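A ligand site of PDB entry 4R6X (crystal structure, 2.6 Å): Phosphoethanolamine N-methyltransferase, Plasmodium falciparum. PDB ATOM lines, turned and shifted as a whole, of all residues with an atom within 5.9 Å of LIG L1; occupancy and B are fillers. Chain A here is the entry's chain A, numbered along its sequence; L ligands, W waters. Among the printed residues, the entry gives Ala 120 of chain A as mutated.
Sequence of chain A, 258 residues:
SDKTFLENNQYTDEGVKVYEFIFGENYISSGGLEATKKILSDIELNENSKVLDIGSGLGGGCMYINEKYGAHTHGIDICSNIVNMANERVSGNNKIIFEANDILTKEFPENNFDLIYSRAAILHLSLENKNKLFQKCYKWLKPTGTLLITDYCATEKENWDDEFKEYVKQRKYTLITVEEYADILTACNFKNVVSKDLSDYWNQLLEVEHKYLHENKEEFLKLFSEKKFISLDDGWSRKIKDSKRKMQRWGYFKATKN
Water W1 lies within hydrogen-bond range of the side-chain hydroxyl (OH) of Tyr 11 (2.6 Å), a nitrogen (N1) of LIG L1 (2.8 Å) and the backbone carbonyl oxygen (O) of Ala 120 (3.1 Å).
NE2 of Gln 248 lies within hydrogen-bond range of OH of Tyr 167, 3.3 Å away.
The side-chain amide nitrogen of Gln 10 lies within hydrogen-bond range of the side-chain hydroxyl of Tyr 173, 2.7 Å away.
NZ of Lys 239 lies within salt-bridge range of O2 of LIG L1, at 3.0 Å.
A sulfur (S1) of LG2 L2 lies close to the side-chain hydroxyl (OH) of Tyr 11 (3.6 Å).
The side-chain amide nitrogen of Gln 10 sits at hydrogen-bond distance from an oxygen (O4) of LIG L1 (3.4 Å).
An oxygen (O2) of LIG L1 sits at hydrogen-bond distance from the side-chain hydroxyl of Tyr 152.
OH of Tyr 167 lies within hydrogen-bond range of O3 of LIG L1, 2.6 Å away.
OG of Ser 29 sits at hydrogen-bond distance from O1 of LG2 L2, 2.4 Å away.
The side-chain hydroxyl (OH) of Tyr 19 is in hydrogen-bond range of an oxygen (O1) of LIG L1 (2.7 Å).
An oxygen (O3) of LIG L1 sits at hydrogen-bond distance from the side-chain hydroxyl (OH) of Tyr 173.
NE of Arg 171 lies within salt-bridge range of O3 of LIG L1 (2.9 Å).
An oxygen (O2) of LG2 L2 sits at hydrogen-bond distance from the backbone NH (N) of Ile 28 (3.0 Å).
The backbone carbonyl oxygen (O) of Ile 28 sits close to a nitrogen (N1) of LIG L1.
Merely in contact with LIG L1: Ala 120 (3.9 Å).
Within 4 Å of LIG L1: Gln 10, Tyr 19, Ile 28, Ala 120, Tyr 152, Tyr 167, Arg 171, Tyr 173 and Lys 239.
The nearest printed residue that does not touch LIG L1 is Phe 23 (4.1 Å).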
ATOM      1  N   GLN A  10       5.938  15.749 -23.943  1.00  0.00           N
ATOM      2  CA  GLN A  10       4.972  15.233 -22.984  1.00  0.00           C
ATOM      3  C   GLN A  10       3.535  15.501 -23.414  1.00  0.00           C
ATOM      4  O   GLN A  10       2.647  14.658 -23.230  1.00  0.00           O
ATOM      5  CB  GLN A  10       5.222  15.826 -21.595  1.00  0.00           C
ATOM      6  CG  GLN A  10       4.342  15.241 -20.492  1.00  0.00           C
ATOM      7  CD  GLN A  10       4.744  15.705 -19.105  1.00  0.00           C
ATOM      8  OE1 GLN A  10       5.584  16.603 -18.961  1.00  0.00           O
ATOM      9  NE2 GLN A  10       4.149  15.104 -18.078  1.00  0.00           N
ATOM     10  N   TYR A  11       3.294  16.668 -24.005  1.00  0.00           N
ATOM     11  CA  TYR A  11       1.936  17.052 -24.374  1.00  0.00           C
ATOM     12  C   TYR A  11       1.738  17.198 -25.884  1.00  0.00           C
ATOM     13  O   TYR A  11       1.256  18.227 -26.352  1.00  0.00           O
ATOM     14  CB  TYR A  11       1.513  18.332 -23.654  1.00  0.00           C
ATOM     15  CG  TYR A  11       1.590  18.228 -22.155  1.00  0.00           C
ATOM     16  CD1 TYR A  11       0.751  17.366 -21.458  1.00  0.00           C
ATOM     17  CD2 TYR A  11       2.498  18.984 -21.419  1.00  0.00           C
ATOM     18  CE1 TYR A  11       0.816  17.256 -20.086  1.00  0.00           C
ATOM     19  CE2 TYR A  11       2.567  18.883 -20.048  1.00  0.00           C
ATOM     20  CZ  TYR A  11       1.718  18.017 -19.382  1.00  0.00           C
ATOM     21  OH  TYR A  11       1.788  17.915 -18.012  1.00  0.00           O
ATOM     22  N   TYR A  19      -2.951  10.047 -22.032  1.00  0.00           N
ATOM     23  CA  TYR A  19      -3.224  10.490 -20.666  1.00  0.00           C
ATOM     24  C   TYR A  19      -4.724  10.517 -20.381  1.00  0.00           C
ATOM     25  O   TYR A  19      -5.168  10.082 -19.318  1.00  0.00           O
ATOM     26  CB  TYR A  19      -2.623  11.877 -20.429  1.00  0.00           C
ATOM     27  CG  TYR A  19      -1.157  11.859 -20.032  1.00  0.00           C
ATOM     28  CD1 TYR A  19      -0.645  10.855 -19.218  1.00  0.00           C
ATOM     29  CD2 TYR A  19      -0.294  12.864 -20.458  1.00  0.00           C
ATOM     30  CE1 TYR A  19       0.695  10.852 -18.855  1.00  0.00           C
ATOM     31  CE2 TYR A  19       1.041  12.862 -20.103  1.00  0.00           C
ATOM     32  CZ  TYR A  19       1.530  11.854 -19.298  1.00  0.00           C
ATOM     33  OH  TYR A  19       2.853  11.848 -18.936  1.00  0.00           O
ATOM     34  N   PHE A  23      -6.874   8.878 -17.357  1.00  0.00           N
ATOM     35  CA  PHE A  23      -7.301   9.886 -16.392  1.00  0.00           C
ATOM     36  C   PHE A  23      -8.808  10.074 -16.400  1.00  0.00           C
ATOM     37  O   PHE A  23      -9.429  10.244 -15.342  1.00  0.00           O
ATOM     38  CB  PHE A  23      -6.597  11.218 -16.680  1.00  0.00           C
ATOM     39  CG  PHE A  23      -5.183  11.286 -16.182  1.00  0.00           C
ATOM     40  CD1 PHE A  23      -4.846  10.789 -14.931  1.00  0.00           C
ATOM     41  CD2 PHE A  23      -4.190  11.838 -16.963  1.00  0.00           C
ATOM     42  CE1 PHE A  23      -3.547  10.854 -14.475  1.00  0.00           C
ATOM     43  CE2 PHE A  23      -2.875  11.907 -16.506  1.00  0.00           C
ATOM     44  CZ  PHE A  23      -2.561  11.406 -15.264  1.00  0.00           C
ATOM     45  N   ILE A  28      -6.156  15.637 -17.681  1.00  0.00           N
ATOM     46  CA  ILE A  28      -4.766  15.224 -17.823  1.00  0.00           C
ATOM     47  C   ILE A  28      -4.089  15.103 -16.447  1.00  0.00           C
ATOM     48  O   ILE A  28      -2.868  15.177 -16.339  1.00  0.00           O
ATOM     49  CB  ILE A  28      -3.947  16.189 -18.719  1.00  0.00           C
ATOM     50  CG1 ILE A  28      -4.846  16.867 -19.768  1.00  0.00           C
ATOM     51  CG2 ILE A  28      -2.804  15.456 -19.411  1.00  0.00           C
ATOM     52  CD1 ILE A  28      -4.098  17.786 -20.702  1.00  0.00           C
ATOM     53  N   SER A  29      -4.892  14.909 -15.403  1.00  0.00           N
ATOM     54  CA  SER A  29      -4.363  14.737 -14.050  1.00  0.00           C
ATOM     55  C   SER A  29      -5.135  13.660 -13.277  1.00  0.00           C
ATOM     56  O   SER A  29      -6.256  13.307 -13.650  1.00  0.00           O
ATOM     57  CB  SER A  29      -4.359  16.059 -13.282  1.00  0.00           C
ATOM     58  OG  SER A  29      -5.666  16.585 -13.168  1.00  0.00           O
ATOM     59  N   SER A  30      -4.529  13.157 -12.211  1.00  0.00           N
ATOM     60  CA  SER A  30      -5.057  11.997 -11.490  1.00  0.00           C
ATOM     61  C   SER A  30      -6.432  12.200 -10.846  1.00  0.00           C
ATOM     62  O   SER A  30      -6.738  13.272 -10.314  1.00  0.00           O
ATOM     63  CB  SER A  30      -4.062  11.503 -10.437  1.00  0.00           C
ATOM     64  OG  SER A  30      -3.116  10.621 -11.013  1.00  0.00           O
ATOM     65  N   ALA A 120      -1.907  20.135 -11.152  1.00  0.00           N
ATOM     66  CA  ALA A 120      -0.789  19.456 -11.812  1.00  0.00           C
ATOM     67  C   ALA A 120      -0.172  20.252 -12.966  1.00  0.00           C
ATOM     68  O   ALA A 120       0.060  19.703 -14.041  1.00  0.00           O
ATOM     69  CB  ALA A 120      -1.215  18.069 -12.291  1.00  0.00           C
ATOM     70  N   LEU A 123       4.205  22.347 -11.436  1.00  0.00           N
ATOM     71  CA  LEU A 123       5.392  21.492 -11.374  1.00  0.00           C
ATOM     72  C   LEU A 123       6.328  21.695 -12.570  1.00  0.00           C
ATOM     73  O   LEU A 123       7.511  21.356 -12.504  1.00  0.00           O
ATOM     74  CB  LEU A 123       5.002  20.023 -11.261  1.00  0.00           C
ATOM     75  CG  LEU A 123       4.626  19.318 -12.569  1.00  0.00           C
ATOM     76  CD1 LEU A 123       4.623  17.819 -12.360  1.00  0.00           C
ATOM     77  CD2 LEU A 123       3.270  19.776 -13.081  1.00  0.00           C
ATOM     78  N   TYR A 152       2.280  17.997  -8.092  1.00  0.00           N
ATOM     79  CA  TYR A 152       3.288  16.994  -7.755  1.00  0.00           C
ATOM     80  C   TYR A 152       4.316  17.593  -6.806  1.00  0.00           C
ATOM     81  O   TYR A 152       4.862  18.668  -7.057  1.00  0.00           O
ATOM     82  CB  TYR A 152       3.994  16.470  -9.011  1.00  0.00           C
ATOM     83  CG  TYR A 152       3.219  15.436  -9.791  1.00  0.00           C
ATOM     84  CD1 TYR A 152       1.939  15.057  -9.411  1.00  0.00           C
ATOM     85  CD2 TYR A 152       3.771  14.837 -10.919  1.00  0.00           C
ATOM     86  CE1 TYR A 152       1.233  14.108 -10.137  1.00  0.00           C
ATOM     87  CE2 TYR A 152       3.077  13.883 -11.642  1.00  0.00           C
ATOM     88  CZ  TYR A 152       1.802  13.530 -11.241  1.00  0.00           C
ATOM     89  OH  TYR A 152       1.107  12.585 -11.974  1.00  0.00           O
ATOM     90  N   TYR A 167      13.513  10.427 -13.903  1.00  0.00           N
ATOM     91  CA  TYR A 167      12.127  10.788 -14.193  1.00  0.00           C
ATOM     92  C   TYR A 167      11.899  12.293 -14.107  1.00  0.00           C
ATOM     93  O   TYR A 167      11.326  12.891 -15.021  1.00  0.00           O
ATOM     94  CB  TYR A 167      11.182  10.043 -13.248  1.00  0.00           C
ATOM     95  CG  TYR A 167       9.788  10.623 -13.168  1.00  0.00           C
ATOM     96  CD1 TYR A 167       8.873  10.419 -14.188  1.00  0.00           C
ATOM     97  CD2 TYR A 167       9.386  11.355 -12.052  1.00  0.00           C
ATOM     98  CE1 TYR A 167       7.593  10.936 -14.106  1.00  0.00           C
ATOM     99  CE2 TYR A 167       8.116  11.879 -11.963  1.00  0.00           C
ATOM    100  CZ  TYR A 167       7.219  11.674 -12.996  1.00  0.00           C
ATOM    101  OH  TYR A 167       5.945  12.190 -12.905  1.00  0.00           O
ATOM    102  N   ARG A 171      11.360  14.804 -17.444  1.00  0.00           N
ATOM    103  CA  ARG A 171      10.106  15.544 -17.454  1.00  0.00           C
ATOM    104  C   ARG A 171      10.363  17.039 -17.327  1.00  0.00           C
ATOM    105  O   ARG A 171       9.463  17.851 -17.553  1.00  0.00           O
ATOM    106  CB  ARG A 171       9.204  15.085 -16.305  1.00  0.00           C
ATOM    107  CG  ARG A 171       8.630  13.691 -16.439  1.00  0.00           C
ATOM    108  CD  ARG A 171       7.578  13.611 -17.529  1.00  0.00           C
ATOM    109  NE  ARG A 171       6.681  12.477 -17.341  1.00  0.00           N
ATOM    110  CZ  ARG A 171       6.912  11.247 -17.792  1.00  0.00           C
ATOM    111  NH1 ARG A 171       8.029  10.985 -18.468  1.00  0.00           N
ATOM    112  NH2 ARG A 171       6.036  10.282 -17.575  1.00  0.00           N
ATOM    113  N   TYR A 173      10.621  18.506 -14.636  1.00  0.00           N
ATOM    114  CA  TYR A 173       9.856  18.940 -13.477  1.00  0.00           C
ATOM    115  C   TYR A 173      10.776  19.646 -12.485  1.00  0.00           C
ATOM    116  O   TYR A 173      11.975  19.374 -12.438  1.00  0.00           O
ATOM    117  CB  TYR A 173       9.213  17.742 -12.763  1.00  0.00           C
ATOM    118  CG  TYR A 173       8.086  17.073 -13.513  1.00  0.00           C
ATOM    119  CD1 TYR A 173       7.471  17.679 -14.591  1.00  0.00           C
ATOM    120  CD2 TYR A 173       7.613  15.826 -13.101  1.00  0.00           C
ATOM    121  CE1 TYR A 173       6.431  17.059 -15.265  1.00  0.00           C
ATOM    122  CE2 TYR A 173       6.575  15.197 -13.765  1.00  0.00           C
ATOM    123  CZ  TYR A 173       5.992  15.820 -14.852  1.00  0.00           C
ATOM    124  OH  TYR A 173       4.959  15.190 -15.507  1.00  0.00           O
ATOM    125  N   TRP A 202      -3.749   9.920  -3.383  1.00  0.00           N
ATOM    126  CA  TRP A 202      -3.228   9.886  -4.742  1.00  0.00           C
ATOM    127  C   TRP A 202      -2.901   8.444  -5.136  1.00  0.00           C
ATOM    128  O   TRP A 202      -3.207   8.010  -6.247  1.00  0.00           O
ATOM    129  CB  TRP A 202      -1.975  10.755  -4.872  1.00  0.00           C
ATOM    130  CG  TRP A 202      -1.403  10.790  -6.264  1.00  0.00           C
ATOM    131  CD1 TRP A 202      -2.106  10.834  -7.430  1.00  0.00           C
ATOM    132  CD2 TRP A 202      -0.024  10.766  -6.622  1.00  0.00           C
ATOM    133  NE1 TRP A 202      -1.242  10.854  -8.501  1.00  0.00           N
ATOM    134  CE2 TRP A 202       0.043  10.817  -8.028  1.00  0.00           C
ATOM    135  CE3 TRP A 202       1.175  10.724  -5.895  1.00  0.00           C
ATOM    136  CZ2 TRP A 202       1.259  10.811  -8.723  1.00  0.00           C
ATOM    137  CZ3 TRP A 202       2.367  10.719  -6.586  1.00  0.00           C
ATOM    138  CH2 TRP A 202       2.406  10.762  -7.985  1.00  0.00           C
ATOM    139  N   TRP A 236       2.817   4.274 -14.269  1.00  0.00           N
ATOM    140  CA  TRP A 236       1.900   4.215 -13.139  1.00  0.00           C
ATOM    141  C   TRP A 236       2.420   3.281 -12.048  1.00  0.00           C
ATOM    142  O   TRP A 236       2.194   3.515 -10.870  1.00  0.00           O
ATOM    143  CB  TRP A 236       0.508   3.792 -13.609  1.00  0.00           C
ATOM    144  CG  TRP A 236      -0.459   4.935 -13.651  1.00  0.00           C
ATOM    145  CD1 TRP A 236      -1.552   5.118 -12.850  1.00  0.00           C
ATOM    146  CD2 TRP A 236      -0.421   6.063 -14.535  1.00  0.00           C
ATOM    147  NE1 TRP A 236      -2.200   6.282 -13.185  1.00  0.00           N
ATOM    148  CE2 TRP A 236      -1.522   6.889 -14.219  1.00  0.00           C
ATOM    149  CE3 TRP A 236       0.439   6.450 -15.560  1.00  0.00           C
ATOM    150  CZ2 TRP A 236      -1.776   8.072 -14.899  1.00  0.00           C
ATOM    151  CZ3 TRP A 236       0.178   7.638 -16.235  1.00  0.00           C
ATOM    152  CH2 TRP A 236      -0.921   8.423 -15.898  1.00  0.00           C
ATOM    153  N   ARG A 238       5.557   2.899 -11.218  1.00  0.00           N
ATOM    154  CA  ARG A 238       6.545   3.664 -10.476  1.00  0.00           C
ATOM    155  C   ARG A 238       5.882   4.707  -9.578  1.00  0.00           C
ATOM    156  O   ARG A 238       6.313   4.919  -8.442  1.00  0.00           O
ATOM    157  CB  ARG A 238       7.546   4.339 -11.415  1.00  0.00           C
ATOM    158  CG  ARG A 238       8.743   4.933 -10.693  1.00  0.00           C
ATOM    159  CD  ARG A 238       9.362   6.067 -11.478  1.00  0.00           C
ATOM    160  NE  ARG A 238       8.359   7.074 -11.831  1.00  0.00           N
ATOM    161  CZ  ARG A 238       7.891   7.997 -11.000  1.00  0.00           C
ATOM    162  NH1 ARG A 238       8.333   8.054  -9.745  1.00  0.00           N
ATOM    163  NH2 ARG A 238       6.991   8.870 -11.418  1.00  0.00           N
ATOM    164  N   LYS A 239       4.839   5.360 -10.090  1.00  0.00           N
ATOM    165  CA  LYS A 239       4.119   6.363  -9.312  1.00  0.00           C
ATOM    166  C   LYS A 239       3.420   5.745  -8.104  1.00  0.00           C
ATOM    167  O   LYS A 239       3.411   6.328  -7.024  1.00  0.00           O
ATOM    168  CB  LYS A 239       3.117   7.127 -10.176  1.00  0.00           C
ATOM    169  CG  LYS A 239       3.772   8.101 -11.153  1.00  0.00           C
ATOM    170  CD  LYS A 239       2.761   9.060 -11.782  1.00  0.00           C
ATOM    171  CE  LYS A 239       1.814   8.332 -12.732  1.00  0.00           C
ATOM    172  NZ  LYS A 239       0.929   9.299 -13.448  1.00  0.00           N
ATOM    173  N   GLN A 248       7.642  10.474  -4.185  1.00  0.00           N
ATOM    174  CA  GLN A 248       6.917  11.409  -5.037  1.00  0.00           C
ATOM    175  C   GLN A 248       5.572  11.691  -4.386  1.00  0.00           C
ATOM    176  O   GLN A 248       4.803  10.769  -4.119  1.00  0.00           O
ATOM    177  CB  GLN A 248       6.722  10.841  -6.451  1.00  0.00           C
ATOM    178  CG  GLN A 248       5.939  11.757  -7.386  1.00  0.00           C
ATOM    179  CD  GLN A 248       5.960  11.287  -8.823  1.00  0.00           C
ATOM    180  OE1 GLN A 248       6.684  10.353  -9.174  1.00  0.00           O
ATOM    181  NE2 GLN A 248       5.173  11.933  -9.670  1.00  0.00           N
HETATM  182  C1  LIG L   1       1.112  13.276 -15.679  1.00  0.00           C
HETATM  183  C2  LIG L   1       0.344  14.525 -15.951  1.00  0.00           C
HETATM  184  O1  LIG L   1       3.217  11.068 -16.342  1.00  0.00           O
HETATM  185  O2  LIG L   1       2.831  11.617 -13.992  1.00  0.00           O
HETATM  186  O3  LIG L   1       4.823  12.562 -15.165  1.00  0.00           O
HETATM  187  O4  LIG L   1       2.490  13.363 -15.715  1.00  0.00           O
HETATM  188  N1  LIG L   1       0.061  15.385 -14.825  1.00  0.00           N
HETATM  189  P1  LIG L   1       3.374  12.154 -15.302  1.00  0.00           P
HETATM  190  N1  LG2 L   2      -5.477  21.234 -15.175  1.00  0.00           N
HETATM  191  C1  LG2 L   2      -5.566  20.157 -16.189  1.00  0.00           C
HETATM  192  C2  LG2 L   2      -4.198  20.011 -16.972  1.00  0.00           C
HETATM  193  C3  LG2 L   2      -3.111  19.155 -16.293  1.00  0.00           C
HETATM  194  S1  LG2 L   2      -1.577  18.846 -17.222  1.00  0.00           S
HETATM  195  C4  LG2 L   2      -6.063  18.926 -15.553  1.00  0.00           C
HETATM  196  O1  LG2 L   2      -5.779  18.692 -14.385  1.00  0.00           O
HETATM  197  O2  LG2 L   2      -6.754  18.158 -16.171  1.00  0.00           O
HETATM  198  C5  LG2 L   2      -0.501  20.298 -17.104  1.00  0.00           C
HETATM  199  C6  LG2 L   2      -0.831  21.463 -17.853  1.00  0.00           C
HETATM  200  O3  LG2 L   2      -0.069  22.573 -17.315  1.00  0.00           O
HETATM  201  C7  LG2 L   2      -0.347  21.279 -19.243  1.00  0.00           C
HETATM  202  O4  LG2 L   2      -1.435  21.246 -20.135  1.00  0.00           O
HETATM  203  C8  LG2 L   2       0.515  22.424 -19.527  1.00  0.00           C
HETATM  204  O5  LG2 L   2       0.165  23.029 -20.740  1.00  0.00           O
HETATM  205  C9  LG2 L   2       0.248  23.377 -18.408  1.00  0.00           C
HETATM  206  N2  LG2 L   2       1.385  24.350 -18.233  1.00  0.00           N
HETATM  207  C10 LG2 L   2       2.679  24.088 -17.985  1.00  0.00           C
HETATM  208  N3  LG2 L   2       3.320  25.265 -17.908  1.00  0.00           N
HETATM  209  C11 LG2 L   2       2.438  26.259 -18.102  1.00  0.00           C
HETATM  210  C12 LG2 L   2       2.551  27.656 -18.123  1.00  0.00           C
HETATM  211  N4  LG2 L   2       3.759  28.262 -17.919  1.00  0.00           N
HETATM  212  N5  LG2 L   2       1.442  28.393 -18.355  1.00  0.00           N
HETATM  213  C13 LG2 L   2       0.257  27.812 -18.550  1.00  0.00           C
HETATM  214  N6  LG2 L   2       0.117  26.462 -18.531  1.00  0.00           N
HETATM  215  C14 LG2 L   2       1.184  25.673 -18.310  1.00  0.00           C
HETATM  216  O   HOH W   1       1.814  17.528 -15.433  1.00  0.00           O
